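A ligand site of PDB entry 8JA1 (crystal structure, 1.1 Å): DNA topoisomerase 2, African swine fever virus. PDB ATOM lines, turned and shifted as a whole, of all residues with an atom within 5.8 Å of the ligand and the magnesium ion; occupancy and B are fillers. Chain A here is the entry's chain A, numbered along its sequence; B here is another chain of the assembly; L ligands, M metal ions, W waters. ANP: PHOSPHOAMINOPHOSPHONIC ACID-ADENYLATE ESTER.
Water W8 bridges OE1 of Glu 60 and ND2 of Asn 64. Water W2 bridges OD2 of Asp 67 (3.3 Å) and N of Gly 142 (3.5 Å). Water W5 lies within hydrogen-bond range of a nitrogen (N7) of the ligand (2.9 Å) and the side-chain amide nitrogen (ND2) of Asn 64 (2.9 Å). Water W4 bridges the backbone carbonyl oxygen of Leu 61 (2.8 Å) and a nitrogen (N6) of the ligand (3.1 Å). Water W1 bridges OD1 of Asn 95 and N6 of the ligand. Water W6 lies within hydrogen-bond range of OE1 of Glu 60 (2.8 Å) and NZ of Lys 368 (3.2 Å).
O of Ala 122 lies within hydrogen-bond range of NZ of Lys 149, at 2.8 Å. ND2 of Asn 64 lies close to O of Glu 60. The side-chain carboxylate (OE2) of Glu 60 is in hydrogen-bond range of the side-chain amide nitrogen (NE2) of Gln 366, 3.1 Å away. NZ of Lys 149 is in hydrogen-bond range of O of Ala 128 (2.9 Å). The side-chain amide oxygen (OE1) of Gln 366 sits at hydrogen-bond distance from the side-chain amide nitrogen (ND2) of Asn 144, at 2.8 Å. The backbone NH (N) of Thr 193 sits at hydrogen-bond distance from the backbone carbonyl oxygen (O) of Asn 95. The backbone carbonyl oxygen (O) of Gly 145 is in hydrogen-bond range of the backbone NH (N) of Ala 128 (3.0 Å). NE2 of His 68 lies within hydrogen-bond range of O of Pro 98 (2.7 Å).
Of the 32 residues printed, 1 comes within 4 Å of the magnesium ion.
The magnesium ion is bound by O2G of the ligand (2.0 Å), water W8 (2.1 Å), OD1 of Asn 64 (2.1 Å), O1B of the ligand (2.1 Å), water W2 (2.1 Å) and O1A of the ligand (2.1 Å).
Residues that only touch the ligand: Glu 60, His 68, Ile 100, Ala 122, Ala 128, Gly 129, Gly 142, Thr 193 and Phe 4 of chain B. Hydrophobic or aromatic side chains that line the ligand: His 68, Ile 100, Ala 122, Val 146, Leu 148 and Phe 4 of chain B.
An oxygen (O3G) of the ligand is in salt-bridge range of the side-chain amino group (NZ) of Lys 368, 2.9 Å away. OD1 of Asn 95 sits at hydrogen-bond distance from N6 of the ligand (2.9 Å). The backbone NH of Asn 144 sits at hydrogen-bond distance from an oxygen (O3G) of the ligand (3.0 Å). O1G of the ligand is in hydrogen-bond range of N of Gly 147 (2.8 Å). The backbone NH (N) of Thr 143 is in hydrogen-bond range of an oxygen (O3G) of the ligand (2.8 Å). O2A of the ligand lies within salt-bridge range of NZ of Lys 149 (2.8 Å). N of Thr 130 is in hydrogen-bond range of O3' of the ligand (3.0 Å). An oxygen (O1G) of the ligand sits at hydrogen-bond distance from the backbone NH (N) of Gly 145 (3.2 Å). An oxygen (O1G) of the ligand is in hydrogen-bond range of the side-chain amide nitrogen (NE2) of Gln 366 (3.2 Å). The side-chain hydroxyl of Thr 130 sits at hydrogen-bond distance from an oxygen (O2') of the ligand (2.8 Å). N of Val 146 is in hydrogen-bond range of O1G of the ligand, 2.7 Å away. An oxygen (O2B) of the ligand lies within hydrogen-bond range of the side-chain amide nitrogen (ND2) of Asn 131, 3.0 Å away. N of Leu 148 lies within hydrogen-bond range of O2A of the ligand.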
ATOM      1  N   GLU A  60     -18.465  22.692  13.489  1.00  0.00           N
ATOM      2  CA  GLU A  60     -18.772  23.942  14.193  1.00  0.00           C
ATOM      3  C   GLU A  60     -20.073  24.541  13.671  1.00  0.00           C
ATOM      4  O   GLU A  60     -20.893  25.036  14.464  1.00  0.00           O
ATOM      5  CB  GLU A  60     -17.625  24.942  14.053  1.00  0.00           C
ATOM      6  CG  GLU A  60     -16.324  24.564  14.759  1.00  0.00           C
ATOM      7  CD  GLU A  60     -16.379  24.508  16.283  1.00  0.00           C
ATOM      8  OE1 GLU A  60     -17.424  24.821  16.893  1.00  0.00           O
ATOM      9  OE2 GLU A  60     -15.338  24.111  16.888  1.00  0.00           O
ATOM     10  N   LEU A  61     -20.283  24.511  12.355  1.00  0.00           N
ATOM     11  CA  LEU A  61     -21.522  25.038  11.778  1.00  0.00           C
ATOM     12  C   LEU A  61     -22.709  24.180  12.177  1.00  0.00           C
ATOM     13  O   LEU A  61     -23.784  24.707  12.503  1.00  0.00           O
ATOM     14  CB  LEU A  61     -21.416  25.111  10.258  1.00  0.00           C
ATOM     15  CG  LEU A  61     -20.897  26.406   9.647  1.00  0.00           C
ATOM     16  CD1 LEU A  61     -19.698  26.927  10.375  1.00  0.00           C
ATOM     17  CD2 LEU A  61     -20.536  26.222   8.189  1.00  0.00           C
ATOM     18  N   VAL A  63     -23.146  22.177  14.849  1.00  0.00           N
ATOM     19  CA  VAL A  63     -23.520  22.365  16.245  1.00  0.00           C
ATOM     20  C   VAL A  63     -24.123  23.743  16.488  1.00  0.00           C
ATOM     21  O   VAL A  63     -25.025  23.896  17.325  1.00  0.00           O
ATOM     22  CB  VAL A  63     -22.325  22.061  17.172  1.00  0.00           C
ATOM     23  CG1 VAL A  63     -22.684  22.306  18.638  1.00  0.00           C
ATOM     24  CG2 VAL A  63     -21.878  20.611  16.979  1.00  0.00           C
ATOM     25  N   ASN A  64     -23.646  24.780  15.788  1.00  0.00           N
ATOM     26  CA  ASN A  64     -24.320  26.068  15.893  1.00  0.00           C
ATOM     27  C   ASN A  64     -25.788  25.967  15.497  1.00  0.00           C
ATOM     28  O   ASN A  64     -26.651  26.599  16.122  1.00  0.00           O
ATOM     29  CB  ASN A  64     -23.623  27.099  15.029  1.00  0.00           C
ATOM     30  CG  ASN A  64     -22.366  27.627  15.676  1.00  0.00           C
ATOM     31  OD1 ASN A  64     -22.153  27.423  16.875  1.00  0.00           O
ATOM     32  ND2 ASN A  64     -21.532  28.325  14.912  1.00  0.00           N
ATOM     33  N   ALA A  65     -26.085  25.187  14.461  1.00  0.00           N
ATOM     34  CA  ALA A  65     -27.475  25.026  14.035  1.00  0.00           C
ATOM     35  C   ALA A  65     -28.275  24.232  15.062  1.00  0.00           C
ATOM     36  O   ALA A  65     -29.401  24.633  15.390  1.00  0.00           O
ATOM     37  CB  ALA A  65     -27.533  24.380  12.652  1.00  0.00           C
ATOM     38  N   ASP A  67     -27.730  24.050  18.168  1.00  0.00           N
ATOM     39  CA  ASP A  67     -27.856  24.873  19.371  1.00  0.00           C
ATOM     40  C   ASP A  67     -29.049  25.822  19.289  1.00  0.00           C
ATOM     41  O   ASP A  67     -29.565  26.258  20.336  1.00  0.00           O
ATOM     42  CB  ASP A  67     -26.606  25.727  19.562  1.00  0.00           C
ATOM     43  CG  ASP A  67     -25.440  25.001  20.205  1.00  0.00           C
ATOM     44  OD1 ASP A  67     -25.576  23.861  20.675  1.00  0.00           O
ATOM     45  OD2 ASP A  67     -24.345  25.640  20.244  1.00  0.00           O
ATOM     46  N   HIS A  68     -29.462  26.213  18.081  1.00  0.00           N
ATOM     47  CA  HIS A  68     -30.340  27.384  17.963  1.00  0.00           C
ATOM     48  C   HIS A  68     -31.710  27.204  18.619  1.00  0.00           C
ATOM     49  O   HIS A  68     -32.245  28.148  19.207  1.00  0.00           O
ATOM     50  CB  HIS A  68     -30.444  27.866  16.521  1.00  0.00           C
ATOM     51  CG  HIS A  68     -30.927  29.276  16.402  1.00  0.00           C
ATOM     52  ND1 HIS A  68     -30.423  30.304  17.174  1.00  0.00           N
ATOM     53  CD2 HIS A  68     -31.866  29.836  15.611  1.00  0.00           C
ATOM     54  CE1 HIS A  68     -31.024  31.432  16.861  1.00  0.00           C
ATOM     55  NE2 HIS A  68     -31.916  31.174  15.914  1.00  0.00           N
ATOM     56  N   ASN A  95     -30.423  27.182   8.992  1.00  0.00           N
ATOM     57  CA  ASN A  95     -31.526  26.854   9.882  1.00  0.00           C
ATOM     58  C   ASN A  95     -32.473  28.039   9.944  1.00  0.00           C
ATOM     59  O   ASN A  95     -32.077  29.185   9.739  1.00  0.00           O
ATOM     60  CB  ASN A  95     -31.059  26.521  11.310  1.00  0.00           C
ATOM     61  CG  ASN A  95     -30.135  27.567  11.916  1.00  0.00           C
ATOM     62  OD1 ASN A  95     -28.933  27.533  11.685  1.00  0.00           O
ATOM     63  ND2 ASN A  95     -30.679  28.464  12.721  1.00  0.00           N
ATOM     64  N   PRO A  98     -35.287  32.530  14.711  1.00  0.00           N
ATOM     65  CA  PRO A  98     -34.897  33.939  14.611  1.00  0.00           C
ATOM     66  C   PRO A  98     -33.499  34.075  14.035  1.00  0.00           C
ATOM     67  O   PRO A  98     -32.585  33.306  14.353  1.00  0.00           O
ATOM     68  CB  PRO A  98     -34.944  34.411  16.077  1.00  0.00           C
ATOM     69  CG  PRO A  98     -35.942  33.513  16.728  1.00  0.00           C
ATOM     70  CD  PRO A  98     -35.754  32.166  16.065  1.00  0.00           C
ATOM     71  N   GLY A  99     -33.332  35.070  13.171  1.00  0.00           N
ATOM     72  CA  GLY A  99     -32.028  35.337  12.620  1.00  0.00           C
ATOM     73  C   GLY A  99     -31.103  35.964  13.655  1.00  0.00           C
ATOM     74  O   GLY A  99     -31.505  36.394  14.740  1.00  0.00           O
ATOM     75  N   ILE A 100     -29.821  36.001  13.303  1.00  0.00           N
ATOM     76  CA  ILE A 100     -28.881  36.786  14.123  1.00  0.00           C
ATOM     77  C   ILE A 100     -29.281  38.253  14.032  1.00  0.00           C
ATOM     78  O   ILE A 100     -29.521  38.750  12.914  1.00  0.00           O
ATOM     79  CB  ILE A 100     -27.442  36.573  13.623  1.00  0.00           C
ATOM     80  CG1 ILE A 100     -27.039  35.095  13.701  1.00  0.00           C
ATOM     81  CG2 ILE A 100     -26.478  37.434  14.424  1.00  0.00           C
ATOM     82  CD1 ILE A 100     -25.642  34.799  13.149  1.00  0.00           C
ATOM     83  N   ALA A 122     -20.404  37.960  15.415  1.00  0.00           N
ATOM     84  CA  ALA A 122     -20.592  36.519  15.571  1.00  0.00           C
ATOM     85  C   ALA A 122     -19.608  35.723  14.734  1.00  0.00           C
ATOM     86  O   ALA A 122     -19.143  34.649  15.159  1.00  0.00           O
ATOM     87  CB  ALA A 122     -22.017  36.143  15.178  1.00  0.00           C
ATOM     88  N   SER A 123     -19.288  36.206  13.541  1.00  0.00           N
ATOM     89  CA  SER A 123     -18.507  35.453  12.565  1.00  0.00           C
ATOM     90  C   SER A 123     -17.051  35.856  12.463  1.00  0.00           C
ATOM     91  O   SER A 123     -16.249  35.061  11.976  1.00  0.00           O
ATOM     92  CB  SER A 123     -19.149  35.582  11.170  1.00  0.00           C
ATOM     93  OG  SER A 123     -19.242  36.962  10.787  1.00  0.00           O
ATOM     94  N   ALA A 128     -16.252  35.699  21.090  1.00  0.00           N
ATOM     95  CA  ALA A 128     -17.453  36.517  21.008  1.00  0.00           C
ATOM     96  C   ALA A 128     -18.655  35.678  20.613  1.00  0.00           C
ATOM     97  O   ALA A 128     -18.587  34.868  19.689  1.00  0.00           O
ATOM     98  CB  ALA A 128     -17.296  37.658  19.991  1.00  0.00           C
ATOM     99  N   GLY A 129     -19.762  35.885  21.324  1.00  0.00           N
ATOM    100  CA  GLY A 129     -20.996  35.162  21.047  1.00  0.00           C
ATOM    101  C   GLY A 129     -21.953  35.324  22.207  1.00  0.00           C
ATOM    102  O   GLY A 129     -21.755  36.176  23.077  1.00  0.00           O
ATOM    103  N   THR A 130     -22.998  34.504  22.218  1.00  0.00           N
ATOM    104  CA  THR A 130     -24.049  34.627  23.227  1.00  0.00           C
ATOM    105  C   THR A 130     -23.863  33.686  24.402  1.00  0.00           C
ATOM    106  O   THR A 130     -24.723  33.661  25.294  1.00  0.00           O
ATOM    107  CB  THR A 130     -25.442  34.426  22.606  1.00  0.00           C
ATOM    108  OG1 THR A 130     -25.480  33.185  21.908  1.00  0.00           O
ATOM    109  CG2 THR A 130     -25.770  35.543  21.644  1.00  0.00           C
ATOM    110  N   ASN A 131     -22.759  32.933  24.443  1.00  0.00           N
ATOM    111  CA  ASN A 131     -22.526  31.944  25.489  1.00  0.00           C
ATOM    112  C   ASN A 131     -21.287  32.241  26.323  1.00  0.00           C
ATOM    113  O   ASN A 131     -20.818  31.360  27.048  1.00  0.00           O
ATOM    114  CB  ASN A 131     -22.465  30.543  24.881  1.00  0.00           C
ATOM    115  CG  ASN A 131     -23.747  30.174  24.193  1.00  0.00           C
ATOM    116  OD1 ASN A 131     -24.807  30.157  24.820  1.00  0.00           O
ATOM    117  ND2 ASN A 131     -23.671  29.918  22.884  1.00  0.00           N
ATOM    118  N   LYS A 140     -26.683  23.957  25.402  1.00  0.00           N
ATOM    119  CA  LYS A 140     -26.062  24.203  24.104  1.00  0.00           C
ATOM    120  C   LYS A 140     -24.645  23.659  24.089  1.00  0.00           C
ATOM    121  O   LYS A 140     -23.937  23.686  25.099  1.00  0.00           O
ATOM    122  CB  LYS A 140     -25.998  25.711  23.819  1.00  0.00           C
ATOM    123  CG  LYS A 140     -27.318  26.350  23.376  1.00  0.00           C
ATOM    124  CD  LYS A 140     -27.132  27.803  22.952  1.00  0.00           C
ATOM    125  CE  LYS A 140     -28.449  28.430  22.496  1.00  0.00           C
ATOM    126  NZ  LYS A 140     -28.289  29.800  21.930  1.00  0.00           N
ATOM    127  N   GLY A 141     -24.227  23.159  22.929  1.00  0.00           N
ATOM    128  CA  GLY A 141     -22.836  22.774  22.769  1.00  0.00           C
ATOM    129  C   GLY A 141     -21.911  23.991  22.795  1.00  0.00           C
ATOM    130  O   GLY A 141     -20.834  23.944  23.394  1.00  0.00           O
ATOM    131  N   GLY A 142     -22.349  25.084  22.190  1.00  0.00           N
ATOM    132  CA  GLY A 142     -21.494  26.262  22.084  1.00  0.00           C
ATOM    133  C   GLY A 142     -21.180  26.873  23.434  1.00  0.00           C
ATOM    134  O   GLY A 142     -22.045  27.016  24.296  1.00  0.00           O
ATOM    135  N   THR A 143     -19.919  27.279  23.597  1.00  0.00           N
ATOM    136  CA  THR A 143     -19.498  27.890  24.849  1.00  0.00           C
ATOM    137  C   THR A 143     -18.436  28.972  24.662  1.00  0.00           C
ATOM    138  O   THR A 143     -18.441  29.950  25.412  1.00  0.00           O
ATOM    139  CB  THR A 143     -19.057  26.851  25.867  1.00  0.00           C
ATOM    140  OG1 THR A 143     -18.627  27.496  27.066  1.00  0.00           O
ATOM    141  CG2 THR A 143     -17.949  26.036  25.329  1.00  0.00           C
ATOM    142  N   ASN A 144     -17.536  28.864  23.672  1.00  0.00           N
ATOM    143  CA  ASN A 144     -16.354  29.703  23.671  1.00  0.00           C
ATOM    144  C   ASN A 144     -16.434  30.984  22.833  1.00  0.00           C
ATOM    145  O   ASN A 144     -15.586  31.872  23.027  1.00  0.00           O
ATOM    146  CB  ASN A 144     -15.140  28.890  23.234  1.00  0.00           C
ATOM    147  CG  ASN A 144     -14.946  27.728  24.137  1.00  0.00           C
ATOM    148  OD1 ASN A 144     -14.949  27.889  25.374  1.00  0.00           O
ATOM    149  ND2 ASN A 144     -14.854  26.540  23.569  1.00  0.00           N
ATOM    150  N   GLY A 145     -17.388  31.109  21.924  1.00  0.00           N
ATOM    151  CA  GLY A 145     -17.333  32.240  21.015  1.00  0.00           C
ATOM    152  C   GLY A 145     -16.207  32.150  20.007  1.00  0.00           C
ATOM    153  O   GLY A 145     -15.681  33.183  19.592  1.00  0.00           O
ATOM    154  N   VAL A 146     -15.881  30.927  19.569  1.00  0.00           N
ATOM    155  CA  VAL A 146     -14.725  30.660  18.717  1.00  0.00           C
ATOM    156  C   VAL A 146     -15.100  29.930  17.432  1.00  0.00           C
ATOM    157  O   VAL A 146     -14.532  30.215  16.373  1.00  0.00           O
ATOM    158  CB  VAL A 146     -13.669  29.848  19.511  1.00  0.00           C
ATOM    159  CG1 VAL A 146     -12.628  29.201  18.596  1.00  0.00           C
ATOM    160  CG2 VAL A 146     -13.016  30.723  20.576  1.00  0.00           C
ATOM    161  N   GLY A 147     -16.031  28.977  17.512  1.00  0.00           N
ATOM    162  CA  GLY A 147     -16.203  28.000  16.437  1.00  0.00           C
ATOM    163  C   GLY A 147     -16.488  28.585  15.060  1.00  0.00           C
ATOM    164  O   GLY A 147     -15.920  28.130  14.065  1.00  0.00           O
ATOM    165  N   LEU A 148     -17.370  29.589  14.978  1.00  0.00           N
ATOM    166  CA  LEU A 148     -17.696  30.155  13.674  1.00  0.00           C
ATOM    167  C   LEU A 148     -16.489  30.880  13.084  1.00  0.00           C
ATOM    168  O   LEU A 148     -16.317  30.887  11.855  1.00  0.00           O
ATOM    169  CB  LEU A 148     -18.912  31.065  13.783  1.00  0.00           C
ATOM    170  CG  LEU A 148     -19.441  31.688  12.479  1.00  0.00           C
ATOM    171  CD1 LEU A 148     -19.674  30.662  11.372  1.00  0.00           C
ATOM    172  CD2 LEU A 148     -20.718  32.432  12.784  1.00  0.00           C
ATOM    173  N   LYS A 149     -15.671  31.487  13.939  1.00  0.00           N
ATOM    174  CA  LYS A 149     -14.476  32.152  13.442  1.00  0.00           C
ATOM    175  C   LYS A 149     -13.493  31.131  12.861  1.00  0.00           C
ATOM    176  O   LYS A 149     -12.812  31.424  11.873  1.00  0.00           O
ATOM    177  CB  LYS A 149     -13.809  32.959  14.548  1.00  0.00           C
ATOM    178  CG  LYS A 149     -14.415  34.356  14.781  1.00  0.00           C
ATOM    179  CD  LYS A 149     -15.864  34.344  15.241  1.00  0.00           C
ATOM    180  CE  LYS A 149     -16.054  33.696  16.599  1.00  0.00           C
ATOM    181  NZ  LYS A 149     -17.378  34.020  17.187  1.00  0.00           N
ATOM    182  N   THR A 193     -30.789  31.715   9.198  1.00  0.00           N
ATOM    183  CA  THR A 193     -29.347  31.953   9.252  1.00  0.00           C
ATOM    184  C   THR A 193     -28.654  30.898   8.403  1.00  0.00           C
ATOM    185  O   THR A 193     -28.891  29.694   8.575  1.00  0.00           O
ATOM    186  CB  THR A 193     -28.804  31.907  10.678  1.00  0.00           C
ATOM    187  OG1 THR A 193     -29.491  32.876  11.482  1.00  0.00           O
ATOM    188  CG2 THR A 193     -27.312  32.228  10.698  1.00  0.00           C
ATOM    189  N   ILE A 195     -24.811  29.827   6.556  1.00  0.00           N
ATOM    190  CA  ILE A 195     -23.375  29.987   6.340  1.00  0.00           C
ATOM    191  C   ILE A 195     -23.014  29.116   5.153  1.00  0.00           C
ATOM    192  O   ILE A 195     -23.320  27.919   5.145  1.00  0.00           O
ATOM    193  CB  ILE A 195     -22.528  29.561   7.561  1.00  0.00           C
ATOM    194  CG1 ILE A 195     -22.996  30.211   8.859  1.00  0.00           C
ATOM    195  CG2 ILE A 195     -21.053  29.842   7.280  1.00  0.00           C
ATOM    196  CD1 ILE A 195     -22.912  31.713   8.911  1.00  0.00           C
ATOM    197  N   GLN A 366     -11.523  23.217  22.627  1.00  0.00           N
ATOM    198  CA  GLN A 366     -12.481  23.739  21.652  1.00  0.00           C
ATOM    199  C   GLN A 366     -13.096  22.632  20.810  1.00  0.00           C
ATOM    200  O   GLN A 366     -14.271  22.730  20.428  1.00  0.00           O
ATOM    201  CB  GLN A 366     -11.818  24.779  20.749  1.00  0.00           C
ATOM    202  CG  GLN A 366     -12.699  25.234  19.581  1.00  0.00           C
ATOM    203  CD  GLN A 366     -13.891  26.077  20.028  1.00  0.00           C
ATOM    204  OE1 GLN A 366     -13.805  26.809  21.017  1.00  0.00           O
ATOM    205  NE2 GLN A 366     -15.007  25.982  19.296  1.00  0.00           N
ATOM    206  N   LYS A 368     -14.080  19.748  21.680  1.00  0.00           N
ATOM    207  CA  LYS A 368     -15.161  19.055  22.379  1.00  0.00           C
ATOM    208  C   LYS A 368     -15.138  17.549  22.090  1.00  0.00           C
ATOM    209  O   LYS A 368     -16.162  16.919  21.811  1.00  0.00           O
ATOM    210  CB  LYS A 368     -16.525  19.684  22.102  1.00  0.00           C
ATOM    211  CG  LYS A 368     -16.517  21.177  22.386  1.00  0.00           C
ATOM    212  CD  LYS A 368     -17.842  21.868  22.060  1.00  0.00           C
ATOM    213  CE  LYS A 368     -17.763  23.363  22.324  1.00  0.00           C
ATOM    214  NZ  LYS A 368     -17.066  24.066  21.223  1.00  0.00           N
ATOM    215  N   PHE B   4     -24.755  39.504  22.602  1.00  0.00           N
ATOM    216  CA  PHE B   4     -23.498  39.094  22.000  1.00  0.00           C
ATOM    217  C   PHE B   4     -22.387  39.844  22.721  1.00  0.00           C
ATOM    218  O   PHE B   4     -22.279  41.065  22.623  1.00  0.00           O
ATOM    219  CB  PHE B   4     -23.486  39.367  20.490  1.00  0.00           C
ATOM    220  CG  PHE B   4     -24.328  38.414  19.680  1.00  0.00           C
ATOM    221  CD1 PHE B   4     -25.717  38.486  19.740  1.00  0.00           C
ATOM    222  CD2 PHE B   4     -23.745  37.444  18.879  1.00  0.00           C
ATOM    223  CE1 PHE B   4     -26.510  37.628  19.012  1.00  0.00           C
ATOM    224  CE2 PHE B   4     -24.540  36.556  18.154  1.00  0.00           C
ATOM    225  CZ  PHE B   4     -25.931  36.649  18.225  1.00  0.00           C
HETATM  226  PG  ANP L   1     -18.221  27.773  20.441  1.00  0.00           P
HETATM  227  O1G ANP L   1     -16.923  28.450  20.137  1.00  0.00           O
HETATM  228  O2G ANP L   1     -18.851  27.196  19.159  1.00  0.00           O
HETATM  229  O3G ANP L   1     -18.052  26.752  21.607  1.00  0.00           O
HETATM  230  PB  ANP L   1     -20.519  29.654  20.191  1.00  0.00           P
HETATM  231  O1B ANP L   1     -21.346  28.720  19.383  1.00  0.00           O
HETATM  232  O2B ANP L   1     -21.320  30.529  21.161  1.00  0.00           O
HETATM  233  N3B ANP L   1     -19.311  28.911  21.089  1.00  0.00           N
HETATM  234  PA  ANP L   1     -19.650  30.632  17.613  1.00  0.00           P
HETATM  235  O1A ANP L   1     -19.781  29.254  17.070  1.00  0.00           O
HETATM  236  O2A ANP L   1     -18.409  31.386  17.234  1.00  0.00           O
HETATM  237  O3A ANP L   1     -19.702  30.603  19.214  1.00  0.00           O
HETATM  238  O5' ANP L   1     -20.959  31.447  17.224  1.00  0.00           O
HETATM  239  C5' ANP L   1     -21.048  32.846  17.604  1.00  0.00           C
HETATM  240  C4' ANP L   1     -22.498  33.154  17.942  1.00  0.00           C
HETATM  241  O4' ANP L   1     -23.242  33.320  16.722  1.00  0.00           O
HETATM  242  C3' ANP L   1     -23.252  32.112  18.748  1.00  0.00           C
HETATM  243  O3' ANP L   1     -23.054  32.303  20.143  1.00  0.00           O
HETATM  244  C2' ANP L   1     -24.709  32.394  18.359  1.00  0.00           C
HETATM  245  O2' ANP L   1     -25.249  33.441  19.154  1.00  0.00           O
HETATM  246  C1' ANP L   1     -24.575  32.875  16.905  1.00  0.00           C
HETATM  247  N9  ANP L   1     -24.846  31.873  15.889  1.00  0.00           N
HETATM  248  C8  ANP L   1     -23.906  31.084  15.274  1.00  0.00           C
HETATM  249  N7  ANP L   1     -24.391  30.264  14.386  1.00  0.00           N
HETATM  250  C5  ANP L   1     -25.757  30.503  14.423  1.00  0.00           C
HETATM  251  C6  ANP L   1     -26.832  29.943  13.716  1.00  0.00           C
HETATM  252  N6  ANP L   1     -26.701  28.960  12.823  1.00  0.00           N
HETATM  253  N1  ANP L   1     -28.078  30.408  13.984  1.00  0.00           N
HETATM  254  C2  ANP L   1     -28.209  31.391  14.877  1.00  0.00           C
HETATM  255  N3  ANP L   1     -27.272  31.986  15.617  1.00  0.00           N
HETATM  256  C4  ANP L   1     -26.047  31.501  15.339  1.00  0.00           C
HETATM  257 MG    MG M   1     -20.434  27.441  18.022  1.00  0.00          MG
HETATM  258  O   HOH W   1     -26.912  27.100   9.936  1.00  0.00           O
HETATM  259  O   HOH W   2     -21.269  25.689  18.926  1.00  0.00           O
HETATM  260  O   HOH W   3     -27.977  32.706  19.398  1.00  0.00           O
HETATM  261  O   HOH W   4     -24.577  27.189  11.483  1.00  0.00           O
HETATM  262  O   HOH W   5     -22.704  29.085  12.387  1.00  0.00           O
HETATM  263  O   HOH W   6     -19.116  23.750  18.800  1.00  0.00           O
HETATM  264  O   HOH W   7     -20.366  32.465  22.861  1.00  0.00           O
HETATM  265  O   HOH W   8     -19.566  26.313  16.527  1.00  0.00           O
HETATM  266  O   HOH W   9     -25.958  28.966  17.487  1.00  0.00           O
HETATM  267  O   HOH W  10     -24.120  28.275  19.475  1.00  0.00           O
